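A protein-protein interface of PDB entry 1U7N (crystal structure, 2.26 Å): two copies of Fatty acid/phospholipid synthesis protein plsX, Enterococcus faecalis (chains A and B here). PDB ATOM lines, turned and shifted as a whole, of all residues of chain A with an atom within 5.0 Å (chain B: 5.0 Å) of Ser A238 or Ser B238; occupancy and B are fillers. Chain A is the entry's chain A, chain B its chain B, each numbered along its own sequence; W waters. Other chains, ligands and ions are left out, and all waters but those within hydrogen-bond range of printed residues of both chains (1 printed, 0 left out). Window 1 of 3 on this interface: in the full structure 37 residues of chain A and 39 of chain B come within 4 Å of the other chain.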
ATOM      1  N   ALA A 214     -17.607  19.039  11.867  1.00  0.00           N
ATOM      2  CA  ALA A 214     -17.896  18.630  13.269  1.00  0.00           C
ATOM      3  C   ALA A 214     -16.856  17.713  13.926  1.00  0.00           C
ATOM      4  O   ALA A 214     -16.702  17.710  15.150  1.00  0.00           O
ATOM      5  CB  ALA A 214     -19.290  18.026  13.403  1.00  0.00           C
ATOM      6  N   ARG A 215     -16.148  16.938  13.116  1.00  0.00           N
ATOM      7  CA  ARG A 215     -15.154  15.982  13.623  1.00  0.00           C
ATOM      8  C   ARG A 215     -13.972  16.703  14.271  1.00  0.00           C
ATOM      9  O   ARG A 215     -13.282  16.152  15.121  1.00  0.00           O
ATOM     10  CB  ARG A 215     -14.651  15.075  12.485  1.00  0.00           C
ATOM     11  CG  ARG A 215     -13.956  13.809  12.983  1.00  0.00           C
ATOM     12  CD  ARG A 215     -13.392  12.911  11.869  1.00  0.00           C
ATOM     13  NE  ARG A 215     -13.516  11.488  12.241  1.00  0.00           N
ATOM     14  CZ  ARG A 215     -12.659  10.799  13.006  1.00  0.00           C
ATOM     15  NH1 ARG A 215     -11.551  11.358  13.499  1.00  0.00           N
ATOM     16  NH2 ARG A 215     -12.912   9.524  13.273  1.00  0.00           N
ATOM     17  N   ASN A 233     -27.562  22.489  19.253  1.00  0.00           N
ATOM     18  CA  ASN A 233     -27.989  21.689  20.400  1.00  0.00           C
ATOM     19  C   ASN A 233     -27.551  20.228  20.228  1.00  0.00           C
ATOM     20  O   ASN A 233     -27.000  19.636  21.150  1.00  0.00           O
ATOM     21  CB  ASN A 233     -29.516  21.783  20.605  1.00  0.00           C
ATOM     22  CG  ASN A 233     -30.039  20.837  21.695  1.00  0.00           C
ATOM     23  OD1 ASN A 233     -29.903  21.107  22.872  1.00  0.00           O
ATOM     24  ND2 ASN A 233     -30.654  19.730  21.288  1.00  0.00           N
ATOM     25  N   ALA A 234     -27.798  19.663  19.049  1.00  0.00           N
ATOM     26  CA  ALA A 234     -27.530  18.251  18.811  1.00  0.00           C
ATOM     27  C   ALA A 234     -26.042  17.921  18.851  1.00  0.00           C
ATOM     28  O   ALA A 234     -25.658  16.902  19.408  1.00  0.00           O
ATOM     29  CB  ALA A 234     -28.151  17.793  17.520  1.00  0.00           C
ATOM     30  N   VAL A 235     -25.229  18.791  18.262  1.00  0.00           N
ATOM     31  CA  VAL A 235     -23.771  18.706  18.291  1.00  0.00           C
ATOM     32  C   VAL A 235     -23.223  18.831  19.715  1.00  0.00           C
ATOM     33  O   VAL A 235     -22.451  17.979  20.151  1.00  0.00           O
ATOM     34  CB  VAL A 235     -23.118  19.780  17.383  1.00  0.00           C
ATOM     35  CG1 VAL A 235     -21.584  19.844  17.625  1.00  0.00           C
ATOM     36  CG2 VAL A 235     -23.417  19.485  15.897  1.00  0.00           C
ATOM     37  N   LEU A 236     -23.603  19.891  20.432  1.00  0.00           N
ATOM     38  CA  LEU A 236     -23.137  20.057  21.800  1.00  0.00           C
ATOM     39  C   LEU A 236     -23.441  18.808  22.640  1.00  0.00           C
ATOM     40  O   LEU A 236     -22.541  18.240  23.243  1.00  0.00           O
ATOM     41  CB  LEU A 236     -23.715  21.327  22.453  1.00  0.00           C
ATOM     42  CG  LEU A 236     -23.286  21.601  23.905  1.00  0.00           C
ATOM     43  CD1 LEU A 236     -21.806  21.851  24.044  1.00  0.00           C
ATOM     44  CD2 LEU A 236     -24.085  22.772  24.496  1.00  0.00           C
ATOM     45  N   LYS A 237     -24.692  18.358  22.637  1.00  0.00           N
ATOM     46  CA  LYS A 237     -25.063  17.220  23.487  1.00  0.00           C
ATOM     47  C   LYS A 237     -24.480  15.875  23.041  1.00  0.00           C
ATOM     48  O   LYS A 237     -24.263  14.998  23.873  1.00  0.00           O
ATOM     49  CB  LYS A 237     -26.569  17.182  23.782  1.00  0.00           C
ATOM     50  CG  LYS A 237     -27.437  16.847  22.626  1.00  0.00           C
ATOM     51  CD  LYS A 237     -28.924  17.200  22.935  1.00  0.00           C
ATOM     52  CE  LYS A 237     -29.854  16.648  21.803  1.00  0.00           C
ATOM     53  NZ  LYS A 237     -31.259  16.442  22.203  1.00  0.00           N
ATOM     54  N   SER A 238     -24.185  15.761  21.741  1.00  0.00           N
ATOM     55  CA  SER A 238     -23.444  14.645  21.157  1.00  0.00           C
ATOM     56  C   SER A 238     -22.026  14.590  21.664  1.00  0.00           C
ATOM     57  O   SER A 238     -21.557  13.523  22.032  1.00  0.00           O
ATOM     58  CB  SER A 238     -23.415  14.718  19.626  1.00  0.00           C
ATOM     59  OG  SER A 238     -24.660  14.351  19.101  1.00  0.00           O
ATOM     60  N   ILE A 239     -21.359  15.743  21.664  1.00  0.00           N
ATOM     61  CA  ILE A 239     -20.040  15.911  22.261  1.00  0.00           C
ATOM     62  C   ILE A 239     -20.055  15.565  23.766  1.00  0.00           C
ATOM     63  O   ILE A 239     -19.213  14.779  24.234  1.00  0.00           O
ATOM     64  CB  ILE A 239     -19.469  17.356  22.035  1.00  0.00           C
ATOM     65  CG1 ILE A 239     -19.124  17.600  20.552  1.00  0.00           C
ATOM     66  CG2 ILE A 239     -18.215  17.620  22.924  1.00  0.00           C
ATOM     67  CD1 ILE A 239     -18.772  19.057  20.227  1.00  0.00           C
ATOM     68  N   GLU A 240     -20.995  16.141  24.519  1.00  0.00           N
ATOM     69  CA  GLU A 240     -21.061  15.872  25.950  1.00  0.00           C
ATOM     70  C   GLU A 240     -21.362  14.395  26.249  1.00  0.00           C
ATOM     71  O   GLU A 240     -20.730  13.808  27.125  1.00  0.00           O
ATOM     72  CB  GLU A 240     -22.065  16.781  26.653  1.00  0.00           C
ATOM     73  CG  GLU A 240     -21.693  18.283  26.565  1.00  0.00           C
ATOM     74  CD  GLU A 240     -22.742  19.173  27.204  1.00  0.00           C
ATOM     75  OE1 GLU A 240     -23.938  18.802  27.159  1.00  0.00           O
ATOM     76  OE2 GLU A 240     -22.375  20.241  27.738  1.00  0.00           O
ATOM     77  N   GLY A 241     -22.305  13.807  25.516  1.00  0.00           N
ATOM     78  CA  GLY A 241     -22.693  12.410  25.729  1.00  0.00           C
ATOM     79  C   GLY A 241     -21.588  11.412  25.442  1.00  0.00           C
ATOM     80  O   GLY A 241     -21.415  10.437  26.172  1.00  0.00           O
ATOM     81  N   THR A 242     -20.835  11.669  24.380  1.00  0.00           N
ATOM     82  CA  THR A 242     -19.687  10.860  23.994  1.00  0.00           C
ATOM     83  C   THR A 242     -18.556  10.986  25.029  1.00  0.00           C
ATOM     84  O   THR A 242     -17.960   9.975  25.449  1.00  0.00           O
ATOM     85  CB  THR A 242     -19.160  11.249  22.581  1.00  0.00           C
ATOM     86  OG1 THR A 242     -20.251  11.328  21.643  1.00  0.00           O
ATOM     87  CG2 THR A 242     -18.074  10.267  22.091  1.00  0.00           C
ATOM     88  N   ALA A 243     -18.239  12.219  25.411  1.00  0.00           N
ATOM     89  CA  ALA A 243     -17.232  12.480  26.452  1.00  0.00           C
ATOM     90  C   ALA A 243     -17.569  11.755  27.750  1.00  0.00           C
ATOM     91  O   ALA A 243     -16.688  11.108  28.329  1.00  0.00           O
ATOM     92  CB  ALA A 243     -17.060  13.970  26.700  1.00  0.00           C
ATOM     93  N   ALA B 214     -29.817  13.528  22.043  1.00  0.00           N
ATOM     94  CA  ALA B 214     -28.518  13.192  21.482  1.00  0.00           C
ATOM     95  C   ALA B 214     -27.483  12.755  22.513  1.00  0.00           C
ATOM     96  O   ALA B 214     -26.556  12.020  22.166  1.00  0.00           O
ATOM     97  CB  ALA B 214     -27.989  14.332  20.637  1.00  0.00           C
ATOM     98  N   ARG B 215     -27.645  13.203  23.764  1.00  0.00           N
ATOM     99  CA  ARG B 215     -26.715  12.866  24.843  1.00  0.00           C
ATOM    100  C   ARG B 215     -26.703  11.361  25.145  1.00  0.00           C
ATOM    101  O   ARG B 215     -25.696  10.814  25.593  1.00  0.00           O
ATOM    102  CB  ARG B 215     -27.039  13.663  26.118  1.00  0.00           C
ATOM    103  CG  ARG B 215     -25.950  13.598  27.165  1.00  0.00           C
ATOM    104  CD  ARG B 215     -26.193  14.509  28.354  1.00  0.00           C
ATOM    105  NE  ARG B 215     -24.916  14.766  29.043  1.00  0.00           N
ATOM    106  CZ  ARG B 215     -24.570  14.258  30.227  1.00  0.00           C
ATOM    107  NH1 ARG B 215     -25.410  13.480  30.905  1.00  0.00           N
ATOM    108  NH2 ARG B 215     -23.385  14.544  30.747  1.00  0.00           N
ATOM    109  N   ASN B 233     -25.450  13.741   9.930  1.00  0.00           N
ATOM    110  CA  ASN B 233     -24.048  13.929   9.650  1.00  0.00           C
ATOM    111  C   ASN B 233     -23.336  14.643  10.791  1.00  0.00           C
ATOM    112  O   ASN B 233     -22.283  14.211  11.235  1.00  0.00           O
ATOM    113  CB  ASN B 233     -23.869  14.760   8.379  1.00  0.00           C
ATOM    114  CG  ASN B 233     -22.407  14.938   8.022  1.00  0.00           C
ATOM    115  OD1 ASN B 233     -21.786  14.024   7.500  1.00  0.00           O
ATOM    116  ND2 ASN B 233     -21.843  16.102   8.338  1.00  0.00           N
ATOM    117  N   ALA B 234     -23.894  15.768  11.235  1.00  0.00           N
ATOM    118  CA  ALA B 234     -23.308  16.526  12.330  1.00  0.00           C
ATOM    119  C   ALA B 234     -23.194  15.695  13.621  1.00  0.00           C
ATOM    120  O   ALA B 234     -22.158  15.735  14.295  1.00  0.00           O
ATOM    121  CB  ALA B 234     -24.080  17.822  12.563  1.00  0.00           C
ATOM    122  N   VAL B 235     -24.245  14.940  13.947  1.00  0.00           N
ATOM    123  CA  VAL B 235     -24.260  14.077  15.132  1.00  0.00           C
ATOM    124  C   VAL B 235     -23.188  12.977  15.018  1.00  0.00           C
ATOM    125  O   VAL B 235     -22.314  12.869  15.879  1.00  0.00           O
ATOM    126  CB  VAL B 235     -25.688  13.529  15.404  1.00  0.00           C
ATOM    127  CG1 VAL B 235     -25.682  12.416  16.443  1.00  0.00           C
ATOM    128  CG2 VAL B 235     -26.648  14.702  15.835  1.00  0.00           C
ATOM    129  N   LEU B 236     -23.211  12.211  13.927  1.00  0.00           N
ATOM    130  CA  LEU B 236     -22.248  11.142  13.733  1.00  0.00           C
ATOM    131  C   LEU B 236     -20.821  11.645  13.843  1.00  0.00           C
ATOM    132  O   LEU B 236     -20.047  11.096  14.618  1.00  0.00           O
ATOM    133  CB  LEU B 236     -22.462  10.411  12.398  1.00  0.00           C
ATOM    134  CG  LEU B 236     -21.537   9.207  12.163  1.00  0.00           C
ATOM    135  CD1 LEU B 236     -21.682   8.156  13.268  1.00  0.00           C
ATOM    136  CD2 LEU B 236     -21.734   8.588  10.777  1.00  0.00           C
ATOM    137  N   LYS B 237     -20.484  12.684  13.084  1.00  0.00           N
ATOM    138  CA  LYS B 237     -19.119  13.210  13.074  1.00  0.00           C
ATOM    139  C   LYS B 237     -18.714  13.843  14.398  1.00  0.00           C
ATOM    140  O   LYS B 237     -17.540  13.833  14.745  1.00  0.00           O
ATOM    141  CB  LYS B 237     -18.900  14.171  11.901  1.00  0.00           C
ATOM    142  CG  LYS B 237     -18.592  13.445  10.587  1.00  0.00           C
ATOM    143  CD  LYS B 237     -18.634  14.386   9.409  1.00  0.00           C
ATOM    144  CE  LYS B 237     -18.659  13.613   8.097  1.00  0.00           C
ATOM    145  NZ  LYS B 237     -19.163  14.449   6.950  1.00  0.00           N
ATOM    146  N   SER B 238     -19.686  14.372  15.135  1.00  0.00           N
ATOM    147  CA  SER B 238     -19.454  14.894  16.497  1.00  0.00           C
ATOM    148  C   SER B 238     -19.061  13.793  17.469  1.00  0.00           C
ATOM    149  O   SER B 238     -18.141  13.970  18.262  1.00  0.00           O
ATOM    150  CB  SER B 238     -20.694  15.589  17.051  1.00  0.00           C
ATOM    151  OG  SER B 238     -20.805  16.856  16.483  1.00  0.00           O
ATOM    152  N   ILE B 239     -19.785  12.677  17.401  1.00  0.00           N
ATOM    153  CA  ILE B 239     -19.481  11.463  18.160  1.00  0.00           C
ATOM    154  C   ILE B 239     -18.083  10.917  17.834  1.00  0.00           C
ATOM    155  O   ILE B 239     -17.266  10.689  18.731  1.00  0.00           O
ATOM    156  CB  ILE B 239     -20.565  10.384  17.932  1.00  0.00           C
ATOM    157  CG1 ILE B 239     -21.904  10.864  18.507  1.00  0.00           C
ATOM    158  CG2 ILE B 239     -20.113   9.020  18.507  1.00  0.00           C
ATOM    159  CD1 ILE B 239     -23.074   9.901  18.343  1.00  0.00           C
ATOM    160  N   GLU B 240     -17.798  10.731  16.558  1.00  0.00           N
ATOM    161  CA  GLU B 240     -16.476  10.258  16.133  1.00  0.00           C
ATOM    162  C   GLU B 240     -15.350  11.186  16.550  1.00  0.00           C
ATOM    163  O   GLU B 240     -14.348  10.727  17.081  1.00  0.00           O
ATOM    164  CB  GLU B 240     -16.433  10.040  14.620  1.00  0.00           C
ATOM    165  CG  GLU B 240     -17.322   8.883  14.167  1.00  0.00           C
ATOM    166  CD  GLU B 240     -17.327   8.695  12.642  1.00  0.00           C
ATOM    167  OE1 GLU B 240     -17.233   9.697  11.899  1.00  0.00           O
ATOM    168  OE2 GLU B 240     -17.457   7.535  12.192  1.00  0.00           O
ATOM    169  N   GLY B 241     -15.514  12.480  16.287  1.00  0.00           N
ATOM    170  CA  GLY B 241     -14.514  13.474  16.640  1.00  0.00           C
ATOM    171  C   GLY B 241     -14.233  13.548  18.134  1.00  0.00           C
ATOM    172  O   GLY B 241     -13.087  13.669  18.550  1.00  0.00           O
ATOM    173  N   THR B 242     -15.284  13.465  18.938  1.00  0.00           N
ATOM    174  CA  THR B 242     -15.143  13.406  20.389  1.00  0.00           C
ATOM    175  C   THR B 242     -14.472  12.116  20.839  1.00  0.00           C
ATOM    176  O   THR B 242     -13.537  12.170  21.633  1.00  0.00           O
ATOM    177  CB  THR B 242     -16.477  13.568  21.097  1.00  0.00           C
ATOM    178  OG1 THR B 242     -17.168  14.697  20.552  1.00  0.00           O
ATOM    179  CG2 THR B 242     -16.265  13.754  22.579  1.00  0.00           C
ATOM    180  N   ALA B 243     -14.930  10.969  20.324  1.00  0.00           N
ATOM    181  CA  ALA B 243     -14.320   9.671  20.675  1.00  0.00           C
ATOM    182  C   ALA B 243     -12.835   9.639  20.334  1.00  0.00           C
ATOM    183  O   ALA B 243     -12.044   9.181  21.150  1.00  0.00           O
ATOM    184  CB  ALA B 243     -15.062   8.494  20.039  1.00  0.00           C
HETATM  185  O   HOH W   1     -18.447  17.993  17.108  1.00  0.00           O
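NZ of Lys A237 sits close to N of Ala B214 (3.3 Å).
OG1 of Thr A242 is in hydrogen-bond range of O of Ser A238 (2.6 Å). OD1 of Asn B233 lies within hydrogen-bond range of NZ of Lys B237 (2.7 Å). The side-chain hydroxyl (OG) of Ser A238 sits at hydrogen-bond distance from the backbone carbonyl oxygen (O) of Ala A234 (2.8 Å). The side-chain hydroxyl (OG) of Ser B238 sits at hydrogen-bond distance from the backbone carbonyl oxygen (O) of Ala B234, 2.8 Å away. The backbone carbonyl oxygen (O) of Ser B238 sits at hydrogen-bond distance from the side-chain hydroxyl (OG1) of Thr B242 (2.6 Å). ND2 of Asn A233 sits close to NZ of Lys A237, 3.5 Å away.
OG of Ser B238 touches CB of Ala A214, at 3.6 Å. Ala A234 touches Val B235 (CB to CG2, 3.8 Å). Ala B234 touches Val A235 (CB to CG2, 3.8 Å). Arg B215 touches Lys A237 (CA to O, 3.4 Å). CB of Ala B214 touches OG of Ser A238, 3.7 Å away. Ser A238 touches Val B235. Ser B238 touches Ser A238. Arg B215 touches Gly A241 (O to CA, 3.4 Å). Thr A242 touches Thr B242 (CG2 to CB, 3.8 Å). Ala A243 touches Thr B242 (N to CG2, 3.8 Å).
Ser B238 touches three residues of chain A. Printed residues of chain B within 4 Å of Ile A239: Thr B242 (3.5 Å). Of the printed residues of chain A, Ala B214 touches Ala A234 (3.7 Å), Lys A237 (3.1 Å) and Ser A238 (3.7 Å). Of the printed residues of chain B, Ala A214 touches Ala B234, Lys B237 and Ser B238. Printed residues of chain A within 4 Å of Arg B215: Lys A237 (3.4 Å) and Gly A241 (3.4 Å). Printed residues of chain B within 4 Å of Lys A237: Ala B214 (3.1 Å) and Arg B215 (3.4 Å). Asn B233 touches none of the printed residues of chain A.
Hydrophobic or aromatic side chains of chain B that line the printed part of chain A: Ala B214, Ala B234, Val B235 and Ile B239.
Arg A215 touches Glu B240, but with the chains exchanged Glu A240 does not touch Arg B215 (4.2 Å). Arg A215 touches Gly B241, and with the chains exchanged Gly A241 touches Arg B215. Ala A234 touches Val B235, and with the chains exchanged Val A235 touches Ala B234. Val A235 touches Ser B238, and with the chains exchanged Ser A238 touches Val B235.
Water W1 lies within hydrogen-bond range of the backbone carbonyl oxygen (O) of Ala A214 (2.6 Å) and the side-chain hydroxyl (OG) of Ser B238 (2.7 Å).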
